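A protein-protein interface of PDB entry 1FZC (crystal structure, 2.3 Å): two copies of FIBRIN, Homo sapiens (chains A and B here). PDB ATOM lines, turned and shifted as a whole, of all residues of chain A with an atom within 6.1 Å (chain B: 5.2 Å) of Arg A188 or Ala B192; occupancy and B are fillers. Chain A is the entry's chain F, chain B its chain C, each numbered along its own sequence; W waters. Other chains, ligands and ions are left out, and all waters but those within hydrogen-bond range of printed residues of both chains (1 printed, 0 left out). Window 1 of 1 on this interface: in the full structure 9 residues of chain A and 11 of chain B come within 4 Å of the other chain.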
ATOM      1  N   LYS A 179     -33.386  -7.951  14.448  1.00  0.00           N
ATOM      2  CA  LYS A 179     -32.672  -7.803  15.708  1.00  0.00           C
ATOM      3  C   LYS A 179     -32.651  -6.309  16.077  1.00  0.00           C
ATOM      4  O   LYS A 179     -32.428  -5.423  15.240  1.00  0.00           O
ATOM      5  CB  LYS A 179     -31.186  -8.241  15.666  1.00  0.00           C
ATOM      6  CG  LYS A 179     -30.994  -9.736  15.787  1.00  0.00           C
ATOM      7  CD  LYS A 179     -29.644 -10.242  15.330  1.00  0.00           C
ATOM      8  CE  LYS A 179     -28.927 -11.088  16.360  1.00  0.00           C
ATOM      9  NZ  LYS A 179     -29.722 -12.227  16.929  1.00  0.00           N
ATOM     10  N   VAL A 180     -32.646  -6.085  17.364  1.00  0.00           N
ATOM     11  CA  VAL A 180     -32.362  -4.805  17.953  1.00  0.00           C
ATOM     12  C   VAL A 180     -31.138  -5.002  18.857  1.00  0.00           C
ATOM     13  O   VAL A 180     -31.091  -5.776  19.837  1.00  0.00           O
ATOM     14  CB  VAL A 180     -33.596  -4.264  18.720  1.00  0.00           C
ATOM     15  CG1 VAL A 180     -33.209  -3.196  19.737  1.00  0.00           C
ATOM     16  CG2 VAL A 180     -34.657  -3.719  17.719  1.00  0.00           C
ATOM     17  N   GLY A 181     -30.141  -4.179  18.614  1.00  0.00           N
ATOM     18  CA  GLY A 181     -28.894  -3.972  19.254  1.00  0.00           C
ATOM     19  C   GLY A 181     -28.988  -3.448  20.682  1.00  0.00           C
ATOM     20  O   GLY A 181     -29.966  -2.900  21.164  1.00  0.00           O
ATOM     21  N   PRO A 182     -27.900  -3.519  21.415  1.00  0.00           N
ATOM     22  CA  PRO A 182     -27.806  -3.056  22.790  1.00  0.00           C
ATOM     23  C   PRO A 182     -27.791  -1.547  22.904  1.00  0.00           C
ATOM     24  O   PRO A 182     -27.476  -0.834  21.936  1.00  0.00           O
ATOM     25  CB  PRO A 182     -26.478  -3.729  23.241  1.00  0.00           C
ATOM     26  CG  PRO A 182     -25.659  -3.721  21.984  1.00  0.00           C
ATOM     27  CD  PRO A 182     -26.647  -4.211  20.931  1.00  0.00           C
ATOM     28  N   ASP A 185     -24.601   0.447  21.438  1.00  0.00           N
ATOM     29  CA  ASP A 185     -24.706   0.836  20.042  1.00  0.00           C
ATOM     30  C   ASP A 185     -26.036   1.585  19.825  1.00  0.00           C
ATOM     31  O   ASP A 185     -26.576   1.613  18.714  1.00  0.00           O
ATOM     32  CB  ASP A 185     -24.520  -0.413  19.166  1.00  0.00           C
ATOM     33  CG  ASP A 185     -24.302  -0.122  17.687  1.00  0.00           C
ATOM     34  OD1 ASP A 185     -23.848   1.000  17.371  1.00  0.00           O
ATOM     35  OD2 ASP A 185     -24.612  -0.967  16.810  1.00  0.00           O
ATOM     36  N   LYS A 186     -26.632   2.200  20.841  1.00  0.00           N
ATOM     37  CA  LYS A 186     -27.941   2.843  20.668  1.00  0.00           C
ATOM     38  C   LYS A 186     -28.943   1.776  20.296  1.00  0.00           C
ATOM     39  O   LYS A 186     -28.675   0.629  20.797  1.00  0.00           O
ATOM     40  CB  LYS A 186     -27.910   3.993  19.687  1.00  0.00           C
ATOM     41  CG  LYS A 186     -26.976   5.136  20.032  1.00  0.00           C
ATOM     42  CD  LYS A 186     -26.856   5.360  21.547  1.00  0.00           C
ATOM     43  CE  LYS A 186     -25.732   6.349  21.833  1.00  0.00           C
ATOM     44  NZ  LYS A 186     -26.282   7.630  22.331  1.00  0.00           N
ATOM     45  N   TYR A 187     -29.985   1.780  19.523  1.00  0.00           N
ATOM     46  CA  TYR A 187     -30.640   0.373  19.687  1.00  0.00           C
ATOM     47  C   TYR A 187     -30.898  -0.027  18.243  1.00  0.00           C
ATOM     48  O   TYR A 187     -32.036   0.064  17.804  1.00  0.00           O
ATOM     49  CB  TYR A 187     -31.902   0.545  20.486  1.00  0.00           C
ATOM     50  CG  TYR A 187     -31.821   0.425  21.982  1.00  0.00           C
ATOM     51  CD1 TYR A 187     -31.622  -0.848  22.551  1.00  0.00           C
ATOM     52  CD2 TYR A 187     -31.930   1.542  22.799  1.00  0.00           C
ATOM     53  CE1 TYR A 187     -31.498  -0.975  23.931  1.00  0.00           C
ATOM     54  CE2 TYR A 187     -31.855   1.384  24.191  1.00  0.00           C
ATOM     55  CZ  TYR A 187     -31.646   0.128  24.738  1.00  0.00           C
ATOM     56  OH  TYR A 187     -31.563  -0.037  26.096  1.00  0.00           O
ATOM     57  N   ARG A 188     -29.753  -0.108  17.588  1.00  0.00           N
ATOM     58  CA  ARG A 188     -29.676  -0.233  16.161  1.00  0.00           C
ATOM     59  C   ARG A 188     -30.643  -1.285  15.650  1.00  0.00           C
ATOM     60  O   ARG A 188     -30.532  -2.375  16.168  1.00  0.00           O
ATOM     61  CB  ARG A 188     -28.258  -0.665  15.714  1.00  0.00           C
ATOM     62  CG  ARG A 188     -28.026  -0.313  14.234  1.00  0.00           C
ATOM     63  CD  ARG A 188     -26.572  -0.597  13.829  1.00  0.00           C
ATOM     64  NE  ARG A 188     -25.553   0.196  14.471  1.00  0.00           N
ATOM     65  CZ  ARG A 188     -25.143   1.398  14.085  1.00  0.00           C
ATOM     66  NH1 ARG A 188     -25.732   1.944  13.003  1.00  0.00           N
ATOM     67  NH2 ARG A 188     -24.165   2.047  14.700  1.00  0.00           N
ATOM     68  N   LEU A 189     -31.430  -0.978  14.639  1.00  0.00           N
ATOM     69  CA  LEU A 189     -32.261  -2.016  14.011  1.00  0.00           C
ATOM     70  C   LEU A 189     -31.435  -2.733  12.926  1.00  0.00           C
ATOM     71  O   LEU A 189     -30.849  -2.077  12.029  1.00  0.00           O
ATOM     72  CB  LEU A 189     -33.455  -1.353  13.344  1.00  0.00           C
ATOM     73  CG  LEU A 189     -34.312  -2.054  12.298  1.00  0.00           C
ATOM     74  CD1 LEU A 189     -35.388  -2.929  12.897  1.00  0.00           C
ATOM     75  CD2 LEU A 189     -35.033  -0.986  11.444  1.00  0.00           C
ATOM     76  N   THR A 190     -31.589  -4.033  12.870  1.00  0.00           N
ATOM     77  CA  THR A 190     -30.875  -4.835  11.887  1.00  0.00           C
ATOM     78  C   THR A 190     -31.839  -5.869  11.335  1.00  0.00           C
ATOM     79  O   THR A 190     -32.662  -6.442  12.075  1.00  0.00           O
ATOM     80  CB  THR A 190     -29.555  -5.403  12.526  1.00  0.00           C
ATOM     81  OG1 THR A 190     -29.546  -6.858  12.544  1.00  0.00           O
ATOM     82  CG2 THR A 190     -29.378  -5.247  14.088  1.00  0.00           C
ATOM     83  N   ASN A 221     -32.864  -0.077   7.521  1.00  0.00           N
ATOM     84  CA  ASN A 221     -31.938  -1.139   7.927  1.00  0.00           C
ATOM     85  C   ASN A 221     -30.595  -0.588   8.412  1.00  0.00           C
ATOM     86  O   ASN A 221     -30.019   0.233   7.717  1.00  0.00           O
ATOM     87  CB  ASN A 221     -31.658  -2.090   6.778  1.00  0.00           C
ATOM     88  CG  ASN A 221     -31.316  -3.495   7.235  1.00  0.00           C
ATOM     89  OD1 ASN A 221     -31.051  -3.757   8.418  1.00  0.00           O
ATOM     90  ND2 ASN A 221     -31.332  -4.449   6.315  1.00  0.00           N
ATOM     91  N   GLY A 222     -30.129  -0.932   9.610  1.00  0.00           N
ATOM     92  CA  GLY A 222     -28.900  -0.453  10.217  1.00  0.00           C
ATOM     93  C   GLY A 222     -29.027   0.881  10.888  1.00  0.00           C
ATOM     94  O   GLY A 222     -27.971   1.453  11.261  1.00  0.00           O
ATOM     95  N   MET A 223     -30.249   1.476  10.948  1.00  0.00           N
ATOM     96  CA  MET A 223     -30.322   2.784  11.622  1.00  0.00           C
ATOM     97  C   MET A 223     -30.285   2.622  13.154  1.00  0.00           C
ATOM     98  O   MET A 223     -30.960   1.703  13.698  1.00  0.00           O
ATOM     99  CB  MET A 223     -31.581   3.565  11.241  1.00  0.00           C
ATOM    100  CG  MET A 223     -31.598   3.987   9.760  1.00  0.00           C
ATOM    101  SD  MET A 223     -30.221   5.092   9.254  1.00  0.00           S
ATOM    102  CE  MET A 223     -29.349   3.865   8.275  1.00  0.00           C
ATOM    103  N   GLN A 224     -29.708   3.604  13.820  1.00  0.00           N
ATOM    104  CA  GLN A 224     -29.739   3.697  15.287  1.00  0.00           C
ATOM    105  C   GLN A 224     -31.091   4.286  15.703  1.00  0.00           C
ATOM    106  O   GLN A 224     -31.767   4.927  14.854  1.00  0.00           O
ATOM    107  CB  GLN A 224     -28.579   4.543  15.877  1.00  0.00           C
ATOM    108  CG  GLN A 224     -27.200   3.882  15.802  1.00  0.00           C
ATOM    109  CD  GLN A 224     -26.001   4.601  16.368  1.00  0.00           C
ATOM    110  OE1 GLN A 224     -25.816   5.809  16.218  1.00  0.00           O
ATOM    111  NE2 GLN A 224     -25.063   3.960  17.095  1.00  0.00           N
ATOM    112  N   PHE A 225     -31.447   4.135  16.995  1.00  0.00           N
ATOM    113  CA  PHE A 225     -32.670   4.654  17.568  1.00  0.00           C
ATOM    114  C   PHE A 225     -32.404   6.110  17.970  1.00  0.00           C
ATOM    115  O   PHE A 225     -31.264   6.362  18.390  1.00  0.00           O
ATOM    116  CB  PHE A 225     -33.277   3.814  18.715  1.00  0.00           C
ATOM    117  CG  PHE A 225     -34.754   4.100  18.980  1.00  0.00           C
ATOM    118  CD1 PHE A 225     -35.192   5.083  19.848  1.00  0.00           C
ATOM    119  CD2 PHE A 225     -35.718   3.309  18.357  1.00  0.00           C
ATOM    120  CE1 PHE A 225     -36.528   5.294  20.080  1.00  0.00           C
ATOM    121  CE2 PHE A 225     -37.068   3.524  18.584  1.00  0.00           C
ATOM    122  CZ  PHE A 225     -37.522   4.502  19.435  1.00  0.00           C
ATOM    123  N   LYS A 234     -29.048  10.499  10.600  1.00  0.00           N
ATOM    124  CA  LYS A 234     -28.064  10.809   9.561  1.00  0.00           C
ATOM    125  C   LYS A 234     -28.277  12.215   9.039  1.00  0.00           C
ATOM    126  O   LYS A 234     -27.970  12.478   7.891  1.00  0.00           O
ATOM    127  CB  LYS A 234     -28.233   9.860   8.334  1.00  0.00           C
ATOM    128  CG  LYS A 234     -27.981   8.389   8.574  1.00  0.00           C
ATOM    129  CD  LYS A 234     -26.665   8.079   9.289  1.00  0.00           C
ATOM    130  CE  LYS A 234     -26.485   6.560   9.410  1.00  0.00           C
ATOM    131  NZ  LYS A 234     -25.399   6.236  10.390  1.00  0.00           N
ATOM    132  N   TRP A 248     -36.252   4.730  14.538  1.00  0.00           N
ATOM    133  CA  TRP A 248     -34.972   4.422  13.877  1.00  0.00           C
ATOM    134  C   TRP A 248     -34.823   5.358  12.690  1.00  0.00           C
ATOM    135  O   TRP A 248     -34.988   4.992  11.531  1.00  0.00           O
ATOM    136  CB  TRP A 248     -35.028   2.922  13.492  1.00  0.00           C
ATOM    137  CG  TRP A 248     -35.015   1.981  14.690  1.00  0.00           C
ATOM    138  CD1 TRP A 248     -33.915   1.704  15.508  1.00  0.00           C
ATOM    139  CD2 TRP A 248     -36.094   1.249  15.216  1.00  0.00           C
ATOM    140  NE1 TRP A 248     -34.277   0.787  16.476  1.00  0.00           N
ATOM    141  CE2 TRP A 248     -35.617   0.499  16.336  1.00  0.00           C
ATOM    142  CE3 TRP A 248     -37.445   1.096  14.842  1.00  0.00           C
ATOM    143  CZ2 TRP A 248     -36.424  -0.371  17.064  1.00  0.00           C
ATOM    144  CZ3 TRP A 248     -38.297   0.214  15.538  1.00  0.00           C
ATOM    145  CH2 TRP A 248     -37.732  -0.446  16.633  1.00  0.00           C
ATOM    146  N   ALA B 176     -20.955  -1.290   6.551  1.00  0.00           N
ATOM    147  CA  ALA B 176     -22.091  -2.145   6.165  1.00  0.00           C
ATOM    148  C   ALA B 176     -23.184  -1.436   5.380  1.00  0.00           C
ATOM    149  O   ALA B 176     -23.521  -0.296   5.750  1.00  0.00           O
ATOM    150  CB  ALA B 176     -22.730  -2.713   7.451  1.00  0.00           C
ATOM    151  N   MET B 177     -23.838  -2.122   4.458  1.00  0.00           N
ATOM    152  CA  MET B 177     -24.921  -1.492   3.682  1.00  0.00           C
ATOM    153  C   MET B 177     -24.373  -0.310   2.850  1.00  0.00           C
ATOM    154  O   MET B 177     -24.924   0.785   2.851  1.00  0.00           O
ATOM    155  CB  MET B 177     -26.035  -0.910   4.515  1.00  0.00           C
ATOM    156  CG  MET B 177     -27.240  -1.751   4.848  1.00  0.00           C
ATOM    157  SD  MET B 177     -26.884  -2.937   6.133  1.00  0.00           S
ATOM    158  CE  MET B 177     -27.643  -2.227   7.562  1.00  0.00           C
ATOM    159  N   THR B 190     -23.339   6.474   0.615  1.00  0.00           N
ATOM    160  CA  THR B 190     -24.140   6.174   1.786  1.00  0.00           C
ATOM    161  C   THR B 190     -23.763   4.776   2.345  1.00  0.00           C
ATOM    162  O   THR B 190     -23.623   3.784   1.605  1.00  0.00           O
ATOM    163  CB  THR B 190     -25.669   6.367   1.696  1.00  0.00           C
ATOM    164  OG1 THR B 190     -26.358   5.105   1.584  1.00  0.00           O
ATOM    165  CG2 THR B 190     -26.267   7.064   0.474  1.00  0.00           C
ATOM    166  N   TYR B 191     -23.755   4.704   3.681  1.00  0.00           N
ATOM    167  CA  TYR B 191     -23.583   3.451   4.416  1.00  0.00           C
ATOM    168  C   TYR B 191     -24.387   3.564   5.734  1.00  0.00           C
ATOM    169  O   TYR B 191     -24.518   4.644   6.372  1.00  0.00           O
ATOM    170  CB  TYR B 191     -22.100   3.111   4.640  1.00  0.00           C
ATOM    171  CG  TYR B 191     -21.362   4.106   5.543  1.00  0.00           C
ATOM    172  CD1 TYR B 191     -21.426   4.007   6.925  1.00  0.00           C
ATOM    173  CD2 TYR B 191     -20.622   5.166   5.028  1.00  0.00           C
ATOM    174  CE1 TYR B 191     -20.820   4.927   7.771  1.00  0.00           C
ATOM    175  CE2 TYR B 191     -20.010   6.083   5.848  1.00  0.00           C
ATOM    176  CZ  TYR B 191     -20.090   5.971   7.210  1.00  0.00           C
ATOM    177  OH  TYR B 191     -19.471   6.897   8.027  1.00  0.00           O
ATOM    178  N   ALA B 192     -24.874   2.513   6.312  1.00  0.00           N
ATOM    179  CA  ALA B 192     -25.517   2.439   7.603  1.00  0.00           C
ATOM    180  C   ALA B 192     -24.566   2.566   8.803  1.00  0.00           C
ATOM    181  O   ALA B 192     -24.744   3.470   9.647  1.00  0.00           O
ATOM    182  CB  ALA B 192     -26.265   1.098   7.753  1.00  0.00           C
ATOM    183  N   TYR B 193     -23.596   1.641   8.924  1.00  0.00           N
ATOM    184  CA  TYR B 193     -22.644   1.666  10.029  1.00  0.00           C
ATOM    185  C   TYR B 193     -21.208   1.198   9.771  1.00  0.00           C
ATOM    186  O   TYR B 193     -20.947   0.353   8.956  1.00  0.00           O
ATOM    187  CB  TYR B 193     -23.198   0.921  11.265  1.00  0.00           C
ATOM    188  CG  TYR B 193     -23.610  -0.528  11.094  1.00  0.00           C
ATOM    189  CD1 TYR B 193     -24.839  -0.866  10.572  1.00  0.00           C
ATOM    190  CD2 TYR B 193     -22.773  -1.576  11.457  1.00  0.00           C
ATOM    191  CE1 TYR B 193     -25.241  -2.168  10.387  1.00  0.00           C
ATOM    192  CE2 TYR B 193     -23.152  -2.896  11.292  1.00  0.00           C
ATOM    193  CZ  TYR B 193     -24.378  -3.191  10.776  1.00  0.00           C
ATOM    194  OH  TYR B 193     -24.813  -4.484  10.574  1.00  0.00           O
ATOM    195  N   PHE B 194     -20.246   1.724  10.520  1.00  0.00           N
ATOM    196  CA  PHE B 194     -18.858   1.305  10.595  1.00  0.00           C
ATOM    197  C   PHE B 194     -18.854  -0.072  11.245  1.00  0.00           C
ATOM    198  O   PHE B 194     -19.425  -0.187  12.338  1.00  0.00           O
ATOM    199  CB  PHE B 194     -17.975   2.283  11.389  1.00  0.00           C
ATOM    200  CG  PHE B 194     -16.576   1.814  11.680  1.00  0.00           C
ATOM    201  CD1 PHE B 194     -15.580   1.857  10.714  1.00  0.00           C
ATOM    202  CD2 PHE B 194     -16.245   1.336  12.960  1.00  0.00           C
ATOM    203  CE1 PHE B 194     -14.308   1.384  10.998  1.00  0.00           C
ATOM    204  CE2 PHE B 194     -14.952   0.874  13.257  1.00  0.00           C
ATOM    205  CZ  PHE B 194     -13.957   0.922  12.266  1.00  0.00           C
ATOM    206  N   ASN B 221     -20.294  10.303   5.286  1.00  0.00           N
ATOM    207  CA  ASN B 221     -21.612   9.718   5.011  1.00  0.00           C
ATOM    208  C   ASN B 221     -22.584  10.740   4.438  1.00  0.00           C
ATOM    209  O   ASN B 221     -22.735  11.823   5.014  1.00  0.00           O
ATOM    210  CB  ASN B 221     -22.180   9.044   6.269  1.00  0.00           C
ATOM    211  CG  ASN B 221     -23.035   7.820   5.970  1.00  0.00           C
ATOM    212  OD1 ASN B 221     -23.341   7.513   4.807  1.00  0.00           O
ATOM    213  ND2 ASN B 221     -23.444   7.146   7.034  1.00  0.00           N
HETATM  214  O   HOH W   1     -22.778   7.719   9.943  1.00  0.00           O
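Among the printed residues, pairs that only touch across the chains: Arg A188 with Tyr B193, Asn A221 with Met B177, Gly A222 with Met B177, Arg A188 with Ala B192, Asn A221 with Ala B192, Lys A234 with Asn B221, Gly A222 with Ala B192 and Gly A222 with Tyr B193.
Of the 17 printed residues of chain A, 4 touch a printed residue of chain B. Printed residues of chain A that touch a printed residue of chain B: Arg A188, Asn A221, Gly A222 and Lys A234. Among the printed residues, no Asp or Glu carboxylate lies within 4 Å of a Lys or Arg side-chain nitrogen of the other chain.
Arg A188 touches just these residues of chain B: Ala B192 and Tyr B193. Printed residues of chain B within 4 Å of Lys A234: Ala B192 (2.9 Å) and Asn B221 (3.9 Å). Printed residues of chain A within 4 Å of Asn B221: Lys A234 (3.9 Å). Of the printed residues of chain A, Met B177 touches Asn A221 (3.4 Å) and Gly A222 (3.4 Å). Printed residues of chain B within 4 Å of Asn A221: Met B177 and Ala B192. Ala B176 touches none of the printed residues of chain A. Met A223 touches none of the printed residues of chain B. The nearest residue of chain A that does not touch Ala B192 is Met A223 (4.1 Å). The nearest printed residue of chain A that does not touch Met B177 is Leu A189 (5.5 Å).
Water W1 bridges ND2 of Asn B221 (3.0 Å) and NZ of Lys A234 (3.0 Å).
The side-chain amino group of Lys A234 is in hydrogen-bond range of the backbone carbonyl oxygen of Ala B192 (2.9 Å).
Positions printed for both chains: 190 and 221.
The backbone carbonyl oxygen (O) of Ala B176 is in hydrogen-bond range of the backbone NH (N) of Ala B192, at 3.2 Å. O of Tyr B193 lies within hydrogen-bond range of N of Ala B176. The side-chain amide nitrogen of Asn B221 lies within hydrogen-bond range of the backbone carbonyl oxygen of Tyr B191 (2.8 Å). O of Arg A188 sits at hydrogen-bond distance from N of Gly A181. The guanidinium group of Arg A188 sits close to the side-chain amide nitrogen of Gln A224, at 3.2 Å. The backbone carbonyl oxygen (O) of Leu A189 is in hydrogen-bond range of the backbone NH (N) of Gly A222, at 2.8 Å.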
